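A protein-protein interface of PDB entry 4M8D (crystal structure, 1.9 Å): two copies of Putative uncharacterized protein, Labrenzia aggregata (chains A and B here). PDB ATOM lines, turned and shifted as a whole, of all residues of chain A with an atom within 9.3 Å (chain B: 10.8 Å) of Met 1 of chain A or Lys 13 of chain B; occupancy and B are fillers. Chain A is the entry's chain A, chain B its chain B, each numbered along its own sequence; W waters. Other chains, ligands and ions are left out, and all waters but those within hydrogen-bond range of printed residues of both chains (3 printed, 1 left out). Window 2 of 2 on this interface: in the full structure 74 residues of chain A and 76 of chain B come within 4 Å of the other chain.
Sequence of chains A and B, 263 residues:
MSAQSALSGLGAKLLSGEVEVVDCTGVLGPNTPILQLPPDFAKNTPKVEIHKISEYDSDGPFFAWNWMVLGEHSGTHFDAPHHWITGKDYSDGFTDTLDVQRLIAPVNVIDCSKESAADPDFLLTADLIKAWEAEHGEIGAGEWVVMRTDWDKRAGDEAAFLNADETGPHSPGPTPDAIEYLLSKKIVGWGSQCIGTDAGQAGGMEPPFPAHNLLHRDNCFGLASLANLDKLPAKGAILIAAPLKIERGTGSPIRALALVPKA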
ATOM      1  N   MET A   1     -25.033 -35.698  -3.727  1.00  0.00           N
ATOM      2  CA  MET A   1     -25.156 -34.372  -3.130  1.00  0.00           C
ATOM      3  C   MET A   1     -23.991 -34.096  -2.179  1.00  0.00           C
ATOM      4  O   MET A   1     -23.850 -32.993  -1.679  1.00  0.00           O
ATOM      5  CB  MET A   1     -26.491 -34.239  -2.397  1.00  0.00           C
ATOM      6  CG  MET A   1     -27.708 -34.641  -3.244  1.00  0.00           C
ATOM      7  SD  MET A   1     -28.339 -33.285  -4.255  1.00  0.00           S
ATOM      8  CE  MET A   1     -28.938 -32.165  -2.990  1.00  0.00           C
ATOM      9  N   SER A   2     -23.167 -35.112  -1.930  1.00  0.00           N
ATOM     10  CA  SER A   2     -21.967 -34.957  -1.117  1.00  0.00           C
ATOM     11  C   SER A   2     -20.834 -34.353  -1.940  1.00  0.00           C
ATOM     12  O   SER A   2     -20.855 -34.399  -3.172  1.00  0.00           O
ATOM     13  CB  SER A   2     -21.516 -36.299  -0.553  1.00  0.00           C
ATOM     14  OG  SER A   2     -20.907 -37.064  -1.573  1.00  0.00           O
ATOM     15  N   ALA A   3     -19.834 -33.810  -1.255  1.00  0.00           N
ATOM     16  CA  ALA A   3     -18.660 -33.273  -1.928  1.00  0.00           C
ATOM     17  C   ALA A   3     -17.936 -34.355  -2.742  1.00  0.00           C
ATOM     18  O   ALA A   3     -17.440 -34.095  -3.834  1.00  0.00           O
ATOM     19  CB  ALA A   3     -17.697 -32.647  -0.907  1.00  0.00           C
ATOM     20  N   GLN A   4     -17.846 -35.561  -2.197  1.00  0.00           N
ATOM     21  CA  GLN A   4     -17.162 -36.631  -2.918  1.00  0.00           C
ATOM     22  C   GLN A   4     -17.911 -36.954  -4.207  1.00  0.00           C
ATOM     23  O   GLN A   4     -17.291 -37.150  -5.261  1.00  0.00           O
ATOM     24  CB  GLN A   4     -17.016 -37.894  -2.065  1.00  0.00           C
ATOM     25  CG  GLN A   4     -16.197 -38.996  -2.770  1.00  0.00           C
ATOM     26  CD  GLN A   4     -14.773 -38.546  -3.111  1.00  0.00           C
ATOM     27  OE1 GLN A   4     -13.897 -38.563  -2.251  1.00  0.00           O
ATOM     28  NE2 GLN A   4     -14.544 -38.141  -4.367  1.00  0.00           N
ATOM     29  N   SER A   5     -19.241 -36.989  -4.133  1.00  0.00           N
ATOM     30  CA  SER A   5     -20.034 -37.255  -5.332  1.00  0.00           C
ATOM     31  C   SER A   5     -19.837 -36.150  -6.344  1.00  0.00           C
ATOM     32  O   SER A   5     -19.772 -36.417  -7.532  1.00  0.00           O
ATOM     33  CB  SER A   5     -21.520 -37.401  -5.015  1.00  0.00           C
ATOM     34  OG  SER A   5     -21.730 -38.538  -4.205  1.00  0.00           O
ATOM     35  N   ALA A   6     -19.737 -34.907  -5.882  1.00  0.00           N
ATOM     36  CA  ALA A   6     -19.503 -33.806  -6.814  1.00  0.00           C
ATOM     37  C   ALA A   6     -18.160 -33.988  -7.536  1.00  0.00           C
ATOM     38  O   ALA A   6     -18.065 -33.820  -8.757  1.00  0.00           O
ATOM     39  CB  ALA A   6     -19.549 -32.456  -6.088  1.00  0.00           C
ATOM     40  N   LEU A   7     -17.128 -34.343  -6.786  1.00  0.00           N
ATOM     41  CA  LEU A   7     -15.804 -34.495  -7.372  1.00  0.00           C
ATOM     42  C   LEU A   7     -15.708 -35.723  -8.284  1.00  0.00           C
ATOM     43  O   LEU A   7     -15.082 -35.660  -9.342  1.00  0.00           O
ATOM     44  CB  LEU A   7     -14.746 -34.568  -6.278  1.00  0.00           C
ATOM     45  CG  LEU A   7     -14.583 -33.241  -5.519  1.00  0.00           C
ATOM     46  CD1 LEU A   7     -13.531 -33.367  -4.400  1.00  0.00           C
ATOM     47  CD2 LEU A   7     -14.242 -32.069  -6.459  1.00  0.00           C
ATOM     48  N   GLY A   9     -18.268 -37.115  -9.829  1.00  0.00           N
ATOM     49  CA  GLY A   9     -19.063 -36.672 -10.960  1.00  0.00           C
ATOM     50  C   GLY A   9     -18.300 -35.766 -11.923  1.00  0.00           C
ATOM     51  O   GLY A   9     -18.387 -35.922 -13.146  1.00  0.00           O
ATOM     52  N   GLN A 101      -8.313 -21.155  -1.765  1.00  0.00           N
ATOM     53  CA  GLN A 101      -9.743 -21.451  -1.830  1.00  0.00           C
ATOM     54  C   GLN A 101     -10.475 -20.431  -2.706  1.00  0.00           C
ATOM     55  O   GLN A 101     -11.411 -20.785  -3.426  1.00  0.00           O
ATOM     56  CB  GLN A 101     -10.360 -21.467  -0.411  1.00  0.00           C
ATOM     57  CG  GLN A 101     -11.824 -21.962  -0.337  1.00  0.00           C
ATOM     58  CD  GLN A 101     -11.926 -23.462  -0.611  1.00  0.00           C
ATOM     59  OE1 GLN A 101     -11.028 -24.215  -0.255  1.00  0.00           O
ATOM     60  NE2 GLN A 101     -13.020 -23.894  -1.239  1.00  0.00           N
ATOM     61  N   ILE A 104     -10.830 -20.409  -7.268  1.00  0.00           N
ATOM     62  CA  ILE A 104     -11.709 -21.200  -8.138  1.00  0.00           C
ATOM     63  C   ILE A 104     -13.148 -20.932  -7.732  1.00  0.00           C
ATOM     64  O   ILE A 104     -13.542 -21.245  -6.616  1.00  0.00           O
ATOM     65  CB  ILE A 104     -11.380 -22.714  -8.025  1.00  0.00           C
ATOM     66  CG1 ILE A 104      -9.887 -22.939  -8.303  1.00  0.00           C
ATOM     67  CG2 ILE A 104     -12.253 -23.563  -8.977  1.00  0.00           C
ATOM     68  CD1 ILE A 104      -9.451 -24.425  -8.154  1.00  0.00           C
ATOM     69  N   ALA A 105     -13.931 -20.321  -8.613  1.00  0.00           N
ATOM     70  CA  ALA A 105     -15.269 -19.911  -8.230  1.00  0.00           C
ATOM     71  C   ALA A 105     -16.172 -19.796  -9.442  1.00  0.00           C
ATOM     72  O   ALA A 105     -15.674 -19.608 -10.564  1.00  0.00           O
ATOM     73  CB  ALA A 105     -15.210 -18.572  -7.474  1.00  0.00           C
ATOM     74  N   PRO A 106     -17.502 -19.898  -9.223  1.00  0.00           N
ATOM     75  CA  PRO A 106     -18.424 -19.513 -10.292  1.00  0.00           C
ATOM     76  C   PRO A 106     -18.065 -18.145 -10.870  1.00  0.00           C
ATOM     77  O   PRO A 106     -17.655 -17.233 -10.122  1.00  0.00           O
ATOM     78  CB  PRO A 106     -19.786 -19.471  -9.583  1.00  0.00           C
ATOM     79  CG  PRO A 106     -19.646 -20.543  -8.510  1.00  0.00           C
ATOM     80  CD  PRO A 106     -18.217 -20.406  -8.035  1.00  0.00           C
ATOM     81  N   ILE A 238     -17.433 -22.307 -14.035  1.00  0.00           N
ATOM     82  CA  ILE A 238     -16.481 -22.140 -12.944  1.00  0.00           C
ATOM     83  C   ILE A 238     -15.150 -21.672 -13.528  1.00  0.00           C
ATOM     84  O   ILE A 238     -14.630 -22.281 -14.470  1.00  0.00           O
ATOM     85  CB  ILE A 238     -16.280 -23.461 -12.171  1.00  0.00           C
ATOM     86  CG1 ILE A 238     -17.602 -23.869 -11.490  1.00  0.00           C
ATOM     87  CG2 ILE A 238     -15.160 -23.318 -11.147  1.00  0.00           C
ATOM     88  CD1 ILE A 238     -17.604 -25.308 -10.890  1.00  0.00           C
ATOM     89  N   SER B   2     -27.650 -33.026 -14.970  1.00  0.00           N
ATOM     90  CA  SER B   2     -26.999 -32.549 -16.186  1.00  0.00           C
ATOM     91  C   SER B   2     -25.659 -31.913 -15.841  1.00  0.00           C
ATOM     92  O   SER B   2     -25.296 -31.786 -14.657  1.00  0.00           O
ATOM     93  CB  SER B   2     -27.881 -31.540 -16.937  1.00  0.00           C
ATOM     94  OG  SER B   2     -27.814 -30.235 -16.358  1.00  0.00           O
ATOM     95  N   SER B   5     -26.192 -28.477 -13.963  1.00  0.00           N
ATOM     96  CA  SER B   5     -26.580 -28.674 -12.569  1.00  0.00           C
ATOM     97  C   SER B   5     -25.383 -29.132 -11.739  1.00  0.00           C
ATOM     98  O   SER B   5     -25.172 -28.652 -10.613  1.00  0.00           O
ATOM     99  CB  SER B   5     -27.725 -29.674 -12.465  1.00  0.00           C
ATOM    100  OG  SER B   5     -28.874 -29.133 -13.084  1.00  0.00           O
ATOM    101  N   ALA B   6     -24.583 -30.031 -12.307  1.00  0.00           N
ATOM    102  CA  ALA B   6     -23.370 -30.485 -11.635  1.00  0.00           C
ATOM    103  C   ALA B   6     -22.416 -29.325 -11.359  1.00  0.00           C
ATOM    104  O   ALA B   6     -21.857 -29.219 -10.263  1.00  0.00           O
ATOM    105  CB  ALA B   6     -22.671 -31.551 -12.463  1.00  0.00           C
ATOM    106  N   LEU B   7     -22.218 -28.446 -12.339  1.00  0.00           N
ATOM    107  CA  LEU B   7     -21.281 -27.347 -12.131  1.00  0.00           C
ATOM    108  C   LEU B   7     -21.831 -26.325 -11.125  1.00  0.00           C
ATOM    109  O   LEU B   7     -21.068 -25.724 -10.377  1.00  0.00           O
ATOM    110  CB  LEU B   7     -20.929 -26.667 -13.464  1.00  0.00           C
ATOM    111  CG  LEU B   7     -20.053 -27.498 -14.414  1.00  0.00           C
ATOM    112  CD1 LEU B   7     -19.821 -26.746 -15.721  1.00  0.00           C
ATOM    113  CD2 LEU B   7     -18.716 -27.852 -13.762  1.00  0.00           C
ATOM    114  N   SER B   8     -23.148 -26.133 -11.105  1.00  0.00           N
ATOM    115  CA  SER B   8     -23.768 -25.251 -10.112  1.00  0.00           C
ATOM    116  C   SER B   8     -23.556 -25.788  -8.698  1.00  0.00           C
ATOM    117  O   SER B   8     -23.175 -25.042  -7.791  1.00  0.00           O
ATOM    118  CB  SER B   8     -25.264 -25.086 -10.406  1.00  0.00           C
ATOM    119  OG  SER B   8     -25.414 -24.523 -11.702  1.00  0.00           O
ATOM    120  N   GLY B   9     -23.778 -27.092  -8.535  1.00  0.00           N
ATOM    121  CA  GLY B   9     -23.607 -27.764  -7.263  1.00  0.00           C
ATOM    122  C   GLY B   9     -22.161 -27.700  -6.817  1.00  0.00           C
ATOM    123  O   GLY B   9     -21.880 -27.387  -5.663  1.00  0.00           O
ATOM    124  N   LEU B  10     -21.243 -27.986  -7.739  1.00  0.00           N
ATOM    125  CA  LEU B  10     -19.818 -27.894  -7.440  1.00  0.00           C
ATOM    126  C   LEU B  10     -19.402 -26.459  -7.096  1.00  0.00           C
ATOM    127  O   LEU B  10     -18.619 -26.240  -6.165  1.00  0.00           O
ATOM    128  CB  LEU B  10     -18.979 -28.414  -8.618  1.00  0.00           C
ATOM    129  CG  LEU B  10     -17.460 -28.312  -8.408  1.00  0.00           C
ATOM    130  CD1 LEU B  10     -17.024 -29.108  -7.173  1.00  0.00           C
ATOM    131  CD2 LEU B  10     -16.688 -28.788  -9.638  1.00  0.00           C
ATOM    132  N   GLY B  11     -19.926 -25.489  -7.848  1.00  0.00           N
ATOM    133  CA  GLY B  11     -19.607 -24.095  -7.606  1.00  0.00           C
ATOM    134  C   GLY B  11     -20.007 -23.664  -6.204  1.00  0.00           C
ATOM    135  O   GLY B  11     -19.260 -22.961  -5.522  1.00  0.00           O
ATOM    136  N   ALA B  12     -21.187 -24.087  -5.772  1.00  0.00           N
ATOM    137  CA  ALA B  12     -21.673 -23.729  -4.442  1.00  0.00           C
ATOM    138  C   ALA B  12     -20.781 -24.331  -3.343  1.00  0.00           C
ATOM    139  O   ALA B  12     -20.549 -23.706  -2.301  1.00  0.00           O
ATOM    140  CB  ALA B  12     -23.119 -24.180  -4.263  1.00  0.00           C
ATOM    141  N   LYS B  13     -20.287 -25.541  -3.585  1.00  0.00           N
ATOM    142  CA  LYS B  13     -19.460 -26.242  -2.611  1.00  0.00           C
ATOM    143  C   LYS B  13     -18.060 -25.642  -2.536  1.00  0.00           C
ATOM    144  O   LYS B  13     -17.440 -25.659  -1.476  1.00  0.00           O
ATOM    145  CB  LYS B  13     -19.384 -27.741  -2.950  1.00  0.00           C
ATOM    146  CG  LYS B  13     -20.641 -28.526  -2.550  1.00  0.00           C
ATOM    147  CD  LYS B  13     -20.564 -29.981  -3.036  1.00  0.00           C
ATOM    148  CE  LYS B  13     -21.709 -30.834  -2.488  1.00  0.00           C
ATOM    149  NZ  LYS B  13     -23.041 -30.378  -2.979  1.00  0.00           N
ATOM    150  N   LEU B  14     -17.556 -25.121  -3.653  1.00  0.00           N
ATOM    151  CA  LEU B  14     -16.277 -24.428  -3.647  1.00  0.00           C
ATOM    152  C   LEU B  14     -16.399 -23.130  -2.850  1.00  0.00           C
ATOM    153  O   LEU B  14     -15.562 -22.831  -2.001  1.00  0.00           O
ATOM    154  CB  LEU B  14     -15.813 -24.131  -5.068  1.00  0.00           C
ATOM    155  CG  LEU B  14     -15.329 -25.356  -5.840  1.00  0.00           C
ATOM    156  CD1 LEU B  14     -15.388 -25.101  -7.339  1.00  0.00           C
ATOM    157  CD2 LEU B  14     -13.899 -25.703  -5.381  1.00  0.00           C
ATOM    158  N   LEU B  15     -17.452 -22.366  -3.126  1.00  0.00           N
ATOM    159  CA  LEU B  15     -17.683 -21.105  -2.415  1.00  0.00           C
ATOM    160  C   LEU B  15     -17.853 -21.326  -0.915  1.00  0.00           C
ATOM    161  O   LEU B  15     -17.440 -20.496  -0.107  1.00  0.00           O
ATOM    162  CB  LEU B  15     -18.927 -20.390  -2.966  1.00  0.00           C
ATOM    163  CG  LEU B  15     -18.795 -19.773  -4.359  1.00  0.00           C
ATOM    164  CD1 LEU B  15     -20.149 -19.274  -4.865  1.00  0.00           C
ATOM    165  CD2 LEU B  15     -17.774 -18.635  -4.339  1.00  0.00           C
ATOM    166  N   SER B  16     -18.484 -22.435  -0.543  1.00  0.00           N
ATOM    167  CA  SER B  16     -18.789 -22.673   0.869  1.00  0.00           C
ATOM    168  C   SER B  16     -17.653 -23.359   1.611  1.00  0.00           C
ATOM    169  O   SER B  16     -17.671 -23.453   2.835  1.00  0.00           O
ATOM    170  CB  SER B  16     -20.045 -23.521   1.010  1.00  0.00           C
ATOM    171  OG  SER B  16     -19.744 -24.871   0.697  1.00  0.00           O
ATOM    172  N   GLY B  17     -16.681 -23.867   0.860  1.00  0.00           N
ATOM    173  CA  GLY B  17     -15.605 -24.636   1.449  1.00  0.00           C
ATOM    174  C   GLY B  17     -15.919 -26.108   1.666  1.00  0.00           C
ATOM    175  O   GLY B  17     -15.063 -26.836   2.148  1.00  0.00           O
ATOM    176  N   GLU B  18     -17.122 -26.558   1.303  1.00  0.00           N
ATOM    177  CA  GLU B  18     -17.467 -27.987   1.396  1.00  0.00           C
ATOM    178  C   GLU B  18     -16.582 -28.838   0.449  1.00  0.00           C
ATOM    179  O   GLU B  18     -16.380 -30.048   0.665  1.00  0.00           O
ATOM    180  CB  GLU B  18     -18.955 -28.205   1.090  1.00  0.00           C
ATOM    181  CG  GLU B  18     -19.423 -29.619   1.369  1.00  0.00           C
ATOM    182  CD  GLU B  18     -20.929 -29.810   1.213  1.00  0.00           C
ATOM    183  OE1 GLU B  18     -21.659 -28.800   1.176  1.00  0.00           O
ATOM    184  OE2 GLU B  18     -21.378 -30.977   1.132  1.00  0.00           O
ATOM    185  N   VAL B  19     -16.074 -28.198  -0.599  1.00  0.00           N
ATOM    186  CA  VAL B  19     -14.944 -28.736  -1.375  1.00  0.00           C
ATOM    187  C   VAL B  19     -13.753 -27.844  -1.090  1.00  0.00           C
ATOM    188  O   VAL B  19     -13.834 -26.634  -1.302  1.00  0.00           O
ATOM    189  CB  VAL B  19     -15.213 -28.771  -2.895  1.00  0.00           C
ATOM    190  CG1 VAL B  19     -13.897 -28.974  -3.685  1.00  0.00           C
ATOM    191  CG2 VAL B  19     -16.244 -29.854  -3.234  1.00  0.00           C
ATOM    192  N   GLU B  20     -12.658 -28.426  -0.596  1.00  0.00           N
ATOM    193  CA  GLU B  20     -11.513 -27.602  -0.204  1.00  0.00           C
ATOM    194  C   GLU B  20     -10.486 -27.543  -1.328  1.00  0.00           C
ATOM    195  O   GLU B  20     -10.197 -28.553  -1.962  1.00  0.00           O
ATOM    196  CB  GLU B  20     -10.843 -28.123   1.085  1.00  0.00           C
ATOM    197  CG  GLU B  20      -9.598 -27.273   1.446  1.00  0.00           C
ATOM    198  CD  GLU B  20      -8.900 -27.665   2.754  1.00  0.00           C
ATOM    199  OE1 GLU B  20      -9.202 -28.721   3.328  1.00  0.00           O
ATOM    200  OE2 GLU B  20      -8.031 -26.893   3.201  1.00  0.00           O
ATOM    201  N   VAL B  21      -9.970 -26.353  -1.597  1.00  0.00           N
ATOM    202  CA  VAL B  21      -8.870 -26.216  -2.544  1.00  0.00           C
ATOM    203  C   VAL B  21      -7.564 -26.344  -1.759  1.00  0.00           C
ATOM    204  O   VAL B  21      -7.306 -25.564  -0.853  1.00  0.00           O
ATOM    205  CB  VAL B  21      -8.901 -24.864  -3.298  1.00  0.00           C
ATOM    206  CG1 VAL B  21      -7.718 -24.784  -4.283  1.00  0.00           C
ATOM    207  CG2 VAL B  21     -10.219 -24.679  -4.045  1.00  0.00           C
ATOM    208  N   ALA B 258      -5.315 -28.992  -5.667  1.00  0.00           N
ATOM    209  CA  ALA B 258      -6.188 -30.154  -5.628  1.00  0.00           C
ATOM    210  C   ALA B 258      -7.520 -29.793  -5.003  1.00  0.00           C
ATOM    211  O   ALA B 258      -7.578 -28.914  -4.151  1.00  0.00           O
ATOM    212  CB  ALA B 258      -5.539 -31.294  -4.855  1.00  0.00           C
ATOM    213  N   LEU B 259      -8.584 -30.467  -5.438  1.00  0.00           N
ATOM    214  CA  LEU B 259      -9.893 -30.365  -4.787  1.00  0.00           C
ATOM    215  C   LEU B 259     -10.113 -31.581  -3.896  1.00  0.00           C
ATOM    216  O   LEU B 259     -10.044 -32.714  -4.378  1.00  0.00           O
ATOM    217  CB  LEU B 259     -11.016 -30.274  -5.828  1.00  0.00           C
ATOM    218  CG  LEU B 259     -10.781 -29.243  -6.935  1.00  0.00           C
ATOM    219  CD1 LEU B 259     -11.941 -29.221  -7.899  1.00  0.00           C
ATOM    220  CD2 LEU B 259     -10.580 -27.855  -6.309  1.00  0.00           C
ATOM    221  N   VAL B 260     -10.385 -31.360  -2.612  1.00  0.00           N
ATOM    222  CA  VAL B 260     -10.645 -32.470  -1.698  1.00  0.00           C
ATOM    223  C   VAL B 260     -12.000 -32.303  -1.025  1.00  0.00           C
ATOM    224  O   VAL B 260     -12.407 -31.197  -0.676  1.00  0.00           O
ATOM    225  CB  VAL B 260      -9.537 -32.633  -0.608  1.00  0.00           C
ATOM    226  CG1 VAL B 260      -8.162 -32.669  -1.243  1.00  0.00           C
ATOM    227  CG2 VAL B 260      -9.603 -31.526   0.415  1.00  0.00           C
ATOM    228  N   PRO B 261     -12.712 -33.416  -0.830  1.00  0.00           N
ATOM    229  CA  PRO B 261     -14.086 -33.331  -0.322  1.00  0.00           C
ATOM    230  C   PRO B 261     -14.170 -33.244   1.199  1.00  0.00           C
ATOM    231  O   PRO B 261     -13.406 -33.915   1.900  1.00  0.00           O
ATOM    232  CB  PRO B 261     -14.710 -34.641  -0.816  1.00  0.00           C
ATOM    233  CG  PRO B 261     -13.557 -35.594  -0.827  1.00  0.00           C
ATOM    234  CD  PRO B 261     -12.341 -34.790  -1.207  1.00  0.00           C
ATOM    235  N   LYS B 262     -15.085 -32.419   1.699  1.00  0.00           N
ATOM    236  CA  LYS B 262     -15.414 -32.422   3.121  1.00  0.00           C
ATOM    237  C   LYS B 262     -16.873 -32.841   3.310  1.00  0.00           C
ATOM    238  O   LYS B 262     -17.592 -33.060   2.331  1.00  0.00           O
ATOM    239  CB  LYS B 262     -15.148 -31.052   3.744  1.00  0.00           C
ATOM    240  CG  LYS B 262     -13.665 -30.696   3.794  1.00  0.00           C
ATOM    241  CD  LYS B 262     -13.468 -29.316   4.376  1.00  0.00           C
ATOM    242  CE  LYS B 262     -12.025 -29.080   4.813  1.00  0.00           C
ATOM    243  NZ  LYS B 262     -11.817 -27.636   5.168  1.00  0.00           N
ATOM    244  N   ALA B 263     -17.299 -32.969   4.563  1.00  0.00           N
ATOM    245  CA  ALA B 263     -18.652 -33.440   4.877  1.00  0.00           C
ATOM    246  C   ALA B 263     -19.214 -32.740   6.113  1.00  0.00           C
ATOM    247  O   ALA B 263     -18.571 -31.860   6.693  1.00  0.00           O
ATOM    248  CB  ALA B 263     -18.658 -34.958   5.074  1.00  0.00           C
ATOM    249  OXT ALA B 263     -20.324 -33.036   6.563  1.00  0.00           O
HETATM  250  O   HOH W   1     -18.046 -35.875   0.847  1.00  0.00           O
HETATM  251  O   HOH W   2     -20.110 -33.238   1.547  1.00  0.00           O
HETATM  252  O   HOH W   3     -23.699 -31.820   0.887  1.00  0.00           O
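The backbone carbonyl oxygen (O) of Met 1 of chain A lies within hydrogen-bond range of the side-chain amino group (NZ) of Lys 13 of chain B (3.0 Å). The backbone carbonyl oxygen (O) of Leu 14 of chain B lies within hydrogen-bond range of the side-chain amide nitrogen (NE2) of Gln 101 of chain A, at 2.9 Å. NE2 of Gln 101 of chain A sits at hydrogen-bond distance from O of Val 19 of chain B (2.9 Å). The side-chain amide oxygen of Gln 101 of chain A sits at hydrogen-bond distance from the backbone NH of Val 21 of chain B.
Among the printed residues, merely in contact across the chains: Ser 2 of chain A with Lys 13 of chain B (3.7 Å), Ala 3 of chain A with Lys 13 of chain B (3.7 Å), Ala 3 of chain A with Glu 18 of chain B (3.3 Å), Ala 3 of chain A with Val 19 of chain B (3.9 Å), Ala 3 of chain A with Pro 261 of chain B (3.6 Å), Ala 3 of chain A with Lys 262 of chain B (3.3 Å), Gln 4 of chain A with Pro 261 of chain B (3.3 Å), Leu 7 of chain A with Leu 259 of chain B (3.5 Å), Leu 7 of chain A with Val 260 of chain B (3.9 Å), Leu 7 of chain A with Pro 261 of chain B (3.7 Å), Gln 101 of chain A with Gly 17 of chain B (3.8 Å), Gln 101 of chain A with Glu 20 of chain B (3.4 Å), Ile 104 of chain A with Leu 14 of chain B (3.9 Å), Pro 106 of chain A with Gly 11 of chain B (3.7 Å), Pro 106 of chain A with Leu 15 of chain B (3.8 Å), Ile 238 of chain A with Leu 7 of chain B (3.5 Å), Ile 238 of chain A with Leu 10 of chain B (3.8 Å) and Ile 238 of chain A with Gly 11 of chain B (3.8 Å).
Ala 6 of chain A touches none of the printed residues of chain B. Ala 105 of chain A touches none of the printed residues of chain B. Printed residues of chain B within 4 Å of Pro 106 of chain A: Gly 11 (3.7 Å) and Leu 15 (3.8 Å). Of the printed residues of chain A, Leu 10 of chain B touches Ile 238. Gly 11 of chain B touches just these residues of chain A: Pro 106 (3.7 Å) and Ile 238 (3.8 Å). No residue of chain A comes within 4 Å of Ala 12 of chain B. Of chain A, only Met 1 (3.0 Å), Ser 2 (3.7 Å) and Ala 3 (3.7 Å) come within 4 Å of Lys 13 of chain B. Of the printed residues of chain A, Leu 15 of chain B touches Pro 106 (3.8 Å). No residue of chain A comes within 4 Å of Ser 16 of chain B. Of chain A, only Gln 101 comes within 4 Å of Gly 17 of chain B. Of the printed residues of chain A, Glu 18 of chain B touches Ala 3 (3.3 Å). Printed residues of chain A within 4 Å of Pro 261 of chain B: Ala 3 (3.6 Å), Gln 4 (3.3 Å) and Leu 7 (3.7 Å). The nearest printed residue of chain A that does not touch Lys 262 of chain B is Gln 4 of chain A (5.2 Å).
Water W3 bridges OE2 of Glu 18 of chain B and O of Met 1 of chain A. Water W2 lies within hydrogen-bond range of the side-chain carboxylate of Glu 18 of chain B (2.6 Å), the backbone carbonyl oxygen of Lys 262 of chain B (2.6 Å) and the backbone NH of Ala 3 of chain A (2.9 Å). Water W1 lies within hydrogen-bond range of N of Gln 4 of chain A, O of Lys 262 of chain B and N of Ala 3 of chain A.
Positions printed for both chains: 2, 5, 6, 7 and 9.
The backbone carbonyl oxygen (O) of Lys 13 of chain B lies within hydrogen-bond range of the backbone NH (N) of Glu 18 of chain B. OG of Ser 16 of chain B lies within hydrogen-bond range of O of Lys 13 of chain B. The backbone NH of Glu 18 of chain B sits at hydrogen-bond distance from the side-chain hydroxyl of Ser 16 of chain B (3.2 Å). OG of Ser 2 of chain A sits close to N of Gln 4 of chain A. The backbone carbonyl oxygen (O) of Glu 18 of chain B is in hydrogen-bond range of the backbone NH (N) of Lys 262 of chain B. O of Val 260 of chain B is in hydrogen-bond range of N of Glu 20 of chain B, 2.8 Å away.
Of the 13 printed residues of chain A, 9 touch a printed residue of chain B. Hydrophobic or aromatic side chains of chain A within 4 Å of the printed part of chain B: Ala 3, Leu 7, Ile 104, Pro 106 and Ile 238. Of the 24 printed residues of chain B, 15 touch a printed residue of chain A. Printed residues of chain B that touch a printed residue of chain A: Leu 7, Leu 10, Gly 11, Lys 13, Leu 14, Leu 15, Gly 17, Glu 18, Val 19, Glu 20, Val 21, Leu 259, Val 260, Pro 261 and Lys 262. Hydrophobic or aromatic side chains of chain B within 4 Å of the printed part of chain A: Leu 7, Leu 10, Leu 14, Leu 15, Val 19, Val 21, Leu 259 and Pro 261. Among the printed residues, 22 pairs touch across the chains.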
